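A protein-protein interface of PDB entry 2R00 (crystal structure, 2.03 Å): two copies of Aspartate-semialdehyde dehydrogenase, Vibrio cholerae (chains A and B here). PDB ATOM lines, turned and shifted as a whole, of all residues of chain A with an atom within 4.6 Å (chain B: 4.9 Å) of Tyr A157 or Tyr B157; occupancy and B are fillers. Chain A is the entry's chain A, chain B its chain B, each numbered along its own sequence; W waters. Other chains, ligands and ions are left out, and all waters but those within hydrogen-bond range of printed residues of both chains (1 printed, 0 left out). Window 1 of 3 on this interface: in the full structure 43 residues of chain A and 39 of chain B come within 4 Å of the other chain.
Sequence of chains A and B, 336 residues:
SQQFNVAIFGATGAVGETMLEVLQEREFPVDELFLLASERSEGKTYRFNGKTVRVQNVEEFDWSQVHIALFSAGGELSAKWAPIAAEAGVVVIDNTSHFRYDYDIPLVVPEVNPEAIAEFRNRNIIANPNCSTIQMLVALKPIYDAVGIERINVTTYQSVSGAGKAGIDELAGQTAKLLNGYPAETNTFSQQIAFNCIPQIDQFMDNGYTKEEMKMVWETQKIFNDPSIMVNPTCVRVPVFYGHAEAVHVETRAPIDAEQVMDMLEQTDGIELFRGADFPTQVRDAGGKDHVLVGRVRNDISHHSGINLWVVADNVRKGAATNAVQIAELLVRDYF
Water W1 bridges the side-chain hydroxyl of Thr A155 (2.7 Å) and the indole nitrogen of Trp B310 (3.2 Å).
The backbone NH of Val A236 lies within hydrogen-bond range of the backbone carbonyl oxygen of Thr A156 (2.9 Å).
N of Tyr A157 sits at hydrogen-bond distance from O of Ala A245 (2.8 Å).
O of Val A236 lies within hydrogen-bond range of N of Gln A158 (3.3 Å).
The backbone carbonyl oxygen (O) of Tyr B157 sits close to a ring nitrogen (NE2) of His B244.
N of Tyr B157 sits at hydrogen-bond distance from O of Ala B245, 3.1 Å away.
O of Gln B158 lies within hydrogen-bond range of N of Phe B241 (3.4 Å).
Tyr A157 touches its own counterpart, Tyr B157.
Val A236 touches Phe B241, but with the chains exchanged Phe A241 does not touch Val B236 (9.1 Å).
Val A236 touches Trp B310, but with the chains exchanged Trp A310 does not touch Val B236 (4.2 Å).
Positions printed for both chains: 155, 156, 157, 158, 236, 241, 244, 245, 246, 247 and 310.
Of the 5 pairs that touch across the chains among the printed residues, 1 has its exchanged pair printed and touching as well.
Of the printed residues of chain B, Tyr A157 touches Tyr B157 (2.6 Å) and Pro B239 (3.6 Å).
Tyr B157 touches one residue of chain A.
Printed residues of chain A within 4 Å of Pro B239: Tyr A157 (3.6 Å) and Phe A241 (3.7 Å).
Of the printed residues of chain B, Phe A241 touches Pro B239 (3.7 Å).
Printed residues of chain A within 4 Å of Phe B241: Val A236 (3.4 Å).
Printed residues of chain A within 4 Å of Trp B310: Val A236.
Gly A243 touches none of the printed residues of chain B.
Thr B156 touches none of the printed residues of chain A.
The nearest residue of chain B that does not touch Tyr A157 is Phe B241 (4.3 Å).
The nearest printed residue of chain A that does not touch Tyr B157 is Thr A155 (4.6 Å).
OH of Tyr A157 lies within hydrogen-bond range of OH of Tyr B157.
Of the 13 printed residues of chain B, 4 touch a printed residue of chain A.
Printed residues of chain B that touch a printed residue of chain A: Tyr B157, Pro B239, Phe B241 and Trp B310.
Hydrophobic or aromatic side chains of chain B within 4 Å of the printed part of chain A: Tyr B157, Pro B239, Phe B241 and Trp B310.
Of the 13 printed residues of chain A, 3 touch a printed residue of chain B.
Hydrophobic or aromatic side chains of chain A within 4 Å of the printed part of chain B: Tyr A157, Val A236 and Phe A241.
Among the printed residues, 5 pairs touch across the chains.
Among the printed residues, merely in contact across the chains: Val A236 with Phe B241 (3.4 Å), Val A236 with Trp B310 (3.5 Å), Tyr A157 with Pro B239 (3.6 Å) and Phe A241 with Pro B239 (3.7 Å).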
ATOM      1  N   THR A 155       7.605  11.370  17.482  1.00  0.00           N
ATOM      2  CA  THR A 155       8.810  11.909  16.861  1.00  0.00           C
ATOM      3  C   THR A 155       9.724  10.752  16.445  1.00  0.00           C
ATOM      4  O   THR A 155      10.027   9.879  17.268  1.00  0.00           O
ATOM      5  CB  THR A 155       9.568  12.867  17.825  1.00  0.00           C
ATOM      6  OG1 THR A 155       8.702  13.934  18.218  1.00  0.00           O
ATOM      7  CG2 THR A 155      10.799  13.461  17.137  1.00  0.00           C
ATOM      8  N   THR A 156      10.127  10.727  15.171  1.00  0.00           N
ATOM      9  CA  THR A 156      11.049   9.709  14.670  1.00  0.00           C
ATOM     10  C   THR A 156      12.402  10.341  14.403  1.00  0.00           C
ATOM     11  O   THR A 156      12.488  11.516  14.054  1.00  0.00           O
ATOM     12  CB  THR A 156      10.558   9.014  13.356  1.00  0.00           C
ATOM     13  OG1 THR A 156      10.592   9.942  12.258  1.00  0.00           O
ATOM     14  CG2 THR A 156       9.151   8.449  13.515  1.00  0.00           C
ATOM     15  N   TYR A 157      13.451   9.538  14.537  1.00  0.00           N
ATOM     16  CA  TYR A 157      14.812  10.026  14.425  1.00  0.00           C
ATOM     17  C   TYR A 157      15.594   9.121  13.485  1.00  0.00           C
ATOM     18  O   TYR A 157      15.635   7.904  13.673  1.00  0.00           O
ATOM     19  CB  TYR A 157      15.497  10.022  15.795  1.00  0.00           C
ATOM     20  CG  TYR A 157      14.779  10.774  16.888  1.00  0.00           C
ATOM     21  CD1 TYR A 157      13.938  10.110  17.777  1.00  0.00           C
ATOM     22  CD2 TYR A 157      14.968  12.140  17.057  1.00  0.00           C
ATOM     23  CE1 TYR A 157      13.286  10.787  18.807  1.00  0.00           C
ATOM     24  CE2 TYR A 157      14.328  12.834  18.084  1.00  0.00           C
ATOM     25  CZ  TYR A 157      13.485  12.151  18.954  1.00  0.00           C
ATOM     26  OH  TYR A 157      12.835  12.829  19.962  1.00  0.00           O
ATOM     27  N   GLN A 158      16.206   9.730  12.478  1.00  0.00           N
ATOM     28  CA  GLN A 158      17.077   9.030  11.550  1.00  0.00           C
ATOM     29  C   GLN A 158      18.174   9.975  11.079  1.00  0.00           C
ATOM     30  O   GLN A 158      18.030  11.192  11.166  1.00  0.00           O
ATOM     31  CB  GLN A 158      16.280   8.494  10.353  1.00  0.00           C
ATOM     32  CG  GLN A 158      15.549   9.559   9.564  1.00  0.00           C
ATOM     33  CD  GLN A 158      14.530   8.980   8.592  1.00  0.00           C
ATOM     34  OE1 GLN A 158      14.784   7.962   7.941  1.00  0.00           O
ATOM     35  NE2 GLN A 158      13.367   9.625   8.496  1.00  0.00           N
ATOM     36  N   VAL A 236      12.305  13.821  12.249  1.00  0.00           N
ATOM     37  CA  VAL A 236      13.486  14.627  12.525  1.00  0.00           C
ATOM     38  C   VAL A 236      14.743  13.960  11.985  1.00  0.00           C
ATOM     39  O   VAL A 236      14.931  12.744  12.118  1.00  0.00           O
ATOM     40  CB  VAL A 236      13.619  14.876  14.058  1.00  0.00           C
ATOM     41  CG1 VAL A 236      14.966  15.452  14.411  1.00  0.00           C
ATOM     42  CG2 VAL A 236      12.530  15.814  14.528  1.00  0.00           C
ATOM     43  N   VAL A 238      18.751  13.643  12.326  1.00  0.00           N
ATOM     44  CA  VAL A 238      19.835  13.927  13.270  1.00  0.00           C
ATOM     45  C   VAL A 238      21.223  13.902  12.593  1.00  0.00           C
ATOM     46  O   VAL A 238      21.475  13.043  11.737  1.00  0.00           O
ATOM     47  CB  VAL A 238      19.734  13.102  14.611  1.00  0.00           C
ATOM     48  CG1 VAL A 238      18.529  12.168  14.651  1.00  0.00           C
ATOM     49  CG2 VAL A 238      21.045  12.408  14.976  1.00  0.00           C
ATOM     50  N   PHE A 241      23.623   9.337  13.230  1.00  0.00           N
ATOM     51  CA  PHE A 241      22.722   8.386  13.900  1.00  0.00           C
ATOM     52  C   PHE A 241      22.760   6.977  13.298  1.00  0.00           C
ATOM     53  O   PHE A 241      22.507   6.800  12.093  1.00  0.00           O
ATOM     54  CB  PHE A 241      21.282   8.924  13.850  1.00  0.00           C
ATOM     55  CG  PHE A 241      20.423   8.532  15.027  1.00  0.00           C
ATOM     56  CD1 PHE A 241      20.790   8.882  16.328  1.00  0.00           C
ATOM     57  CD2 PHE A 241      19.210   7.867  14.829  1.00  0.00           C
ATOM     58  CE1 PHE A 241      19.982   8.544  17.414  1.00  0.00           C
ATOM     59  CE2 PHE A 241      18.385   7.527  15.911  1.00  0.00           C
ATOM     60  CZ  PHE A 241      18.780   7.868  17.208  1.00  0.00           C
ATOM     61  N   GLY A 243      20.939   3.389  13.429  1.00  0.00           N
ATOM     62  CA  GLY A 243      19.674   2.784  13.801  1.00  0.00           C
ATOM     63  C   GLY A 243      18.567   3.818  13.762  1.00  0.00           C
ATOM     64  O   GLY A 243      18.747   4.927  13.244  1.00  0.00           O
ATOM     65  N   HIS A 244      17.422   3.456  14.323  1.00  0.00           N
ATOM     66  CA  HIS A 244      16.238   4.289  14.250  1.00  0.00           C
ATOM     67  C   HIS A 244      15.537   4.325  15.597  1.00  0.00           C
ATOM     68  O   HIS A 244      15.475   3.316  16.300  1.00  0.00           O
ATOM     69  CB  HIS A 244      15.291   3.749  13.167  1.00  0.00           C
ATOM     70  CG  HIS A 244      14.028   4.535  13.020  1.00  0.00           C
ATOM     71  ND1 HIS A 244      12.826   4.114  13.550  1.00  0.00           N
ATOM     72  CD2 HIS A 244      13.780   5.723  12.418  1.00  0.00           C
ATOM     73  CE1 HIS A 244      11.891   5.007  13.279  1.00  0.00           C
ATOM     74  NE2 HIS A 244      12.444   5.994  12.595  1.00  0.00           N
ATOM     75  N   ALA A 245      15.003   5.487  15.950  1.00  0.00           N
ATOM     76  CA  ALA A 245      14.295   5.636  17.220  1.00  0.00           C
ATOM     77  C   ALA A 245      13.033   6.467  17.045  1.00  0.00           C
ATOM     78  O   ALA A 245      12.941   7.269  16.112  1.00  0.00           O
ATOM     79  CB  ALA A 245      15.205   6.262  18.265  1.00  0.00           C
ATOM     80  N   GLU A 246      12.069   6.255  17.944  1.00  0.00           N
ATOM     81  CA  GLU A 246      10.827   7.019  18.001  1.00  0.00           C
ATOM     82  C   GLU A 246      10.466   7.297  19.440  1.00  0.00           C
ATOM     83  O   GLU A 246      10.576   6.419  20.274  1.00  0.00           O
ATOM     84  CB  GLU A 246       9.671   6.234  17.406  1.00  0.00           C
ATOM     85  CG  GLU A 246       9.928   5.710  16.038  1.00  0.00           C
ATOM     86  CD  GLU A 246       8.801   4.884  15.539  1.00  0.00           C
ATOM     87  OE1 GLU A 246       8.149   4.187  16.344  1.00  0.00           O
ATOM     88  OE2 GLU A 246       8.564   4.933  14.334  1.00  0.00           O
ATOM     89  N   ALA A 247      10.027   8.519  19.711  1.00  0.00           N
ATOM     90  CA  ALA A 247       9.443   8.891  20.993  1.00  0.00           C
ATOM     91  C   ALA A 247       7.942   8.965  20.766  1.00  0.00           C
ATOM     92  O   ALA A 247       7.486   9.639  19.827  1.00  0.00           O
ATOM     93  CB  ALA A 247       9.980  10.250  21.447  1.00  0.00           C
ATOM     94  N   TRP A 310       9.472   5.025  24.354  1.00  0.00           N
ATOM     95  CA  TRP A 310      10.392   5.123  23.232  1.00  0.00           C
ATOM     96  C   TRP A 310      10.574   3.751  22.613  1.00  0.00           C
ATOM     97  O   TRP A 310      10.569   2.738  23.310  1.00  0.00           O
ATOM     98  CB  TRP A 310      11.748   5.666  23.681  1.00  0.00           C
ATOM     99  CG  TRP A 310      11.756   7.160  23.904  1.00  0.00           C
ATOM    100  CD1 TRP A 310      10.974   7.865  24.779  1.00  0.00           C
ATOM    101  CD2 TRP A 310      12.600   8.122  23.256  1.00  0.00           C
ATOM    102  NE1 TRP A 310      11.272   9.208  24.706  1.00  0.00           N
ATOM    103  CE2 TRP A 310      12.270   9.392  23.785  1.00  0.00           C
ATOM    104  CE3 TRP A 310      13.600   8.035  22.276  1.00  0.00           C
ATOM    105  CZ2 TRP A 310      12.906  10.564  23.367  1.00  0.00           C
ATOM    106  CZ3 TRP A 310      14.226   9.193  21.861  1.00  0.00           C
ATOM    107  CH2 TRP A 310      13.884  10.445  22.409  1.00  0.00           C
ATOM    108  N   THR B 155      10.729  17.569  25.304  1.00  0.00           N
ATOM    109  CA  THR B 155      11.973  16.797  25.259  1.00  0.00           C
ATOM    110  C   THR B 155      13.148  17.753  25.070  1.00  0.00           C
ATOM    111  O   THR B 155      13.136  18.556  24.146  1.00  0.00           O
ATOM    112  CB  THR B 155      11.970  15.754  24.129  1.00  0.00           C
ATOM    113  OG1 THR B 155      10.866  14.860  24.305  1.00  0.00           O
ATOM    114  CG2 THR B 155      13.281  14.936  24.149  1.00  0.00           C
ATOM    115  N   THR B 156      14.137  17.687  25.961  1.00  0.00           N
ATOM    116  CA  THR B 156      15.349  18.486  25.830  1.00  0.00           C
ATOM    117  C   THR B 156      16.486  17.585  25.351  1.00  0.00           C
ATOM    118  O   THR B 156      16.567  16.427  25.760  1.00  0.00           O
ATOM    119  CB  THR B 156      15.770  19.154  27.171  1.00  0.00           C
ATOM    120  OG1 THR B 156      16.262  18.149  28.065  1.00  0.00           O
ATOM    121  CG2 THR B 156      14.595  19.854  27.816  1.00  0.00           C
ATOM    122  N   TYR B 157      17.358  18.128  24.498  1.00  0.00           N
ATOM    123  CA  TYR B 157      18.449  17.378  23.875  1.00  0.00           C
ATOM    124  C   TYR B 157      19.768  18.051  24.153  1.00  0.00           C
ATOM    125  O   TYR B 157      19.867  19.277  24.081  1.00  0.00           O
ATOM    126  CB  TYR B 157      18.280  17.320  22.352  1.00  0.00           C
ATOM    127  CG  TYR B 157      16.967  16.774  21.869  1.00  0.00           C
ATOM    128  CD1 TYR B 157      15.882  17.618  21.651  1.00  0.00           C
ATOM    129  CD2 TYR B 157      16.806  15.410  21.611  1.00  0.00           C
ATOM    130  CE1 TYR B 157      14.657  17.118  21.195  1.00  0.00           C
ATOM    131  CE2 TYR B 157      15.585  14.901  21.154  1.00  0.00           C
ATOM    132  CZ  TYR B 157      14.517  15.769  20.957  1.00  0.00           C
ATOM    133  OH  TYR B 157      13.306  15.288  20.517  1.00  0.00           O
ATOM    134  N   GLN B 158      20.792  17.261  24.449  1.00  0.00           N
ATOM    135  CA  GLN B 158      22.137  17.807  24.577  1.00  0.00           C
ATOM    136  C   GLN B 158      22.683  18.204  23.215  1.00  0.00           C
ATOM    137  O   GLN B 158      22.208  17.714  22.182  1.00  0.00           O
ATOM    138  CB  GLN B 158      23.067  16.816  25.271  1.00  0.00           C
ATOM    139  CG  GLN B 158      22.832  16.758  26.775  1.00  0.00           C
ATOM    140  CD  GLN B 158      23.814  15.864  27.495  1.00  0.00           C
ATOM    141  OE1 GLN B 158      24.560  15.097  26.874  1.00  0.00           O
ATOM    142  NE2 GLN B 158      23.810  15.944  28.822  1.00  0.00           N
ATOM    143  N   SER B 159      23.661  19.111  23.218  1.00  0.00           N
ATOM    144  CA  SER B 159      24.272  19.595  21.983  1.00  0.00           C
ATOM    145  C   SER B 159      25.473  18.745  21.573  1.00  0.00           C
ATOM    146  O   SER B 159      26.161  18.184  22.422  1.00  0.00           O
ATOM    147  CB  SER B 159      24.691  21.061  22.135  1.00  0.00           C
ATOM    148  OG  SER B 159      25.286  21.555  20.937  1.00  0.00           O
ATOM    149  N   VAL B 236      17.089  14.148  27.494  1.00  0.00           N
ATOM    150  CA  VAL B 236      17.939  13.134  26.848  1.00  0.00           C
ATOM    151  C   VAL B 236      19.350  13.604  26.438  1.00  0.00           C
ATOM    152  O   VAL B 236      19.617  14.796  26.267  1.00  0.00           O
ATOM    153  CB  VAL B 236      17.222  12.463  25.625  1.00  0.00           C
ATOM    154  CG1 VAL B 236      15.873  11.869  26.033  1.00  0.00           C
ATOM    155  CG2 VAL B 236      17.039  13.431  24.489  1.00  0.00           C
ATOM    156  N   PRO B 239      19.138  11.372  20.897  1.00  0.00           N
ATOM    157  CA  PRO B 239      20.088  11.902  19.926  1.00  0.00           C
ATOM    158  C   PRO B 239      20.528  13.309  20.342  1.00  0.00           C
ATOM    159  O   PRO B 239      19.966  13.889  21.275  1.00  0.00           O
ATOM    160  CB  PRO B 239      19.251  11.984  18.649  1.00  0.00           C
ATOM    161  CG  PRO B 239      17.871  12.298  19.160  1.00  0.00           C
ATOM    162  CD  PRO B 239      17.752  11.402  20.373  1.00  0.00           C
ATOM    163  N   PHE B 241      21.801  17.358  18.778  1.00  0.00           N
ATOM    164  CA  PHE B 241      21.631  18.277  17.653  1.00  0.00           C
ATOM    165  C   PHE B 241      22.634  19.417  17.788  1.00  0.00           C
ATOM    166  O   PHE B 241      23.225  19.593  18.857  1.00  0.00           O
ATOM    167  CB  PHE B 241      20.206  18.839  17.642  1.00  0.00           C
ATOM    168  CG  PHE B 241      19.137  17.798  17.420  1.00  0.00           C
ATOM    169  CD1 PHE B 241      18.807  17.388  16.127  1.00  0.00           C
ATOM    170  CD2 PHE B 241      18.450  17.248  18.497  1.00  0.00           C
ATOM    171  CE1 PHE B 241      17.820  16.424  15.918  1.00  0.00           C
ATOM    172  CE2 PHE B 241      17.449  16.286  18.302  1.00  0.00           C
ATOM    173  CZ  PHE B 241      17.136  15.870  17.012  1.00  0.00           C
ATOM    174  N   HIS B 244      21.206  23.928  21.219  1.00  0.00           N
ATOM    175  CA  HIS B 244      20.475  23.230  22.259  1.00  0.00           C
ATOM    176  C   HIS B 244      18.979  23.194  21.918  1.00  0.00           C
ATOM    177  O   HIS B 244      18.283  24.195  22.034  1.00  0.00           O
ATOM    178  CB  HIS B 244      20.734  23.868  23.631  1.00  0.00           C
ATOM    179  CG  HIS B 244      20.008  23.186  24.750  1.00  0.00           C
ATOM    180  ND1 HIS B 244      18.819  23.661  25.260  1.00  0.00           N
ATOM    181  CD2 HIS B 244      20.286  22.049  25.434  1.00  0.00           C
ATOM    182  CE1 HIS B 244      18.400  22.854  26.217  1.00  0.00           C
ATOM    183  NE2 HIS B 244      19.271  21.868  26.341  1.00  0.00           N
ATOM    184  N   ALA B 245      18.503  22.026  21.487  1.00  0.00           N
ATOM    185  CA  ALA B 245      17.140  21.872  20.985  1.00  0.00           C
ATOM    186  C   ALA B 245      16.156  21.407  22.042  1.00  0.00           C
ATOM    187  O   ALA B 245      16.510  20.636  22.941  1.00  0.00           O
ATOM    188  CB  ALA B 245      17.113  20.915  19.791  1.00  0.00           C
ATOM    189  N   GLU B 246      14.917  21.873  21.904  1.00  0.00           N
ATOM    190  CA  GLU B 246      13.785  21.372  22.676  1.00  0.00           C
ATOM    191  C   GLU B 246      12.582  21.155  21.772  1.00  0.00           C
ATOM    192  O   GLU B 246      12.278  21.980  20.908  1.00  0.00           O
ATOM    193  CB  GLU B 246      13.403  22.339  23.802  1.00  0.00           C
ATOM    194  CG  GLU B 246      14.484  22.520  24.853  1.00  0.00           C
ATOM    195  CD  GLU B 246      14.108  23.525  25.919  1.00  0.00           C
ATOM    196  OE1 GLU B 246      13.048  24.178  25.783  1.00  0.00           O
ATOM    197  OE2 GLU B 246      14.877  23.651  26.899  1.00  0.00           O
ATOM    198  N   ALA B 247      11.888  20.050  21.987  1.00  0.00           N
ATOM    199  CA  ALA B 247      10.663  19.768  21.268  1.00  0.00           C
ATOM    200  C   ALA B 247       9.539  19.935  22.272  1.00  0.00           C
ATOM    201  O   ALA B 247       9.574  19.336  23.354  1.00  0.00           O
ATOM    202  CB  ALA B 247      10.680  18.368  20.719  1.00  0.00           C
ATOM    203  N   TRP B 310       9.336  23.459  17.881  1.00  0.00           N
ATOM    204  CA  TRP B 310      10.721  23.255  18.314  1.00  0.00           C
ATOM    205  C   TRP B 310      11.334  24.582  18.733  1.00  0.00           C
ATOM    206  O   TRP B 310      11.036  25.623  18.146  1.00  0.00           O
ATOM    207  CB  TRP B 310      11.581  22.564  17.235  1.00  0.00           C
ATOM    208  CG  TRP B 310      11.371  21.067  17.192  1.00  0.00           C
ATOM    209  CD1 TRP B 310      10.200  20.420  16.900  1.00  0.00           C
ATOM    210  CD2 TRP B 310      12.336  20.035  17.463  1.00  0.00           C
ATOM    211  NE1 TRP B 310      10.378  19.062  16.967  1.00  0.00           N
ATOM    212  CE2 TRP B 310      11.678  18.795  17.300  1.00  0.00           C
ATOM    213  CE3 TRP B 310      13.691  20.038  17.810  1.00  0.00           C
ATOM    214  CZ2 TRP B 310      12.320  17.567  17.494  1.00  0.00           C
ATOM    215  CZ3 TRP B 310      14.332  18.816  18.003  1.00  0.00           C
ATOM    216  CH2 TRP B 310      13.643  17.596  17.839  1.00  0.00           C
HETATM  217  O   HOH W   1       8.582  16.622  18.082  1.00  0.00           O
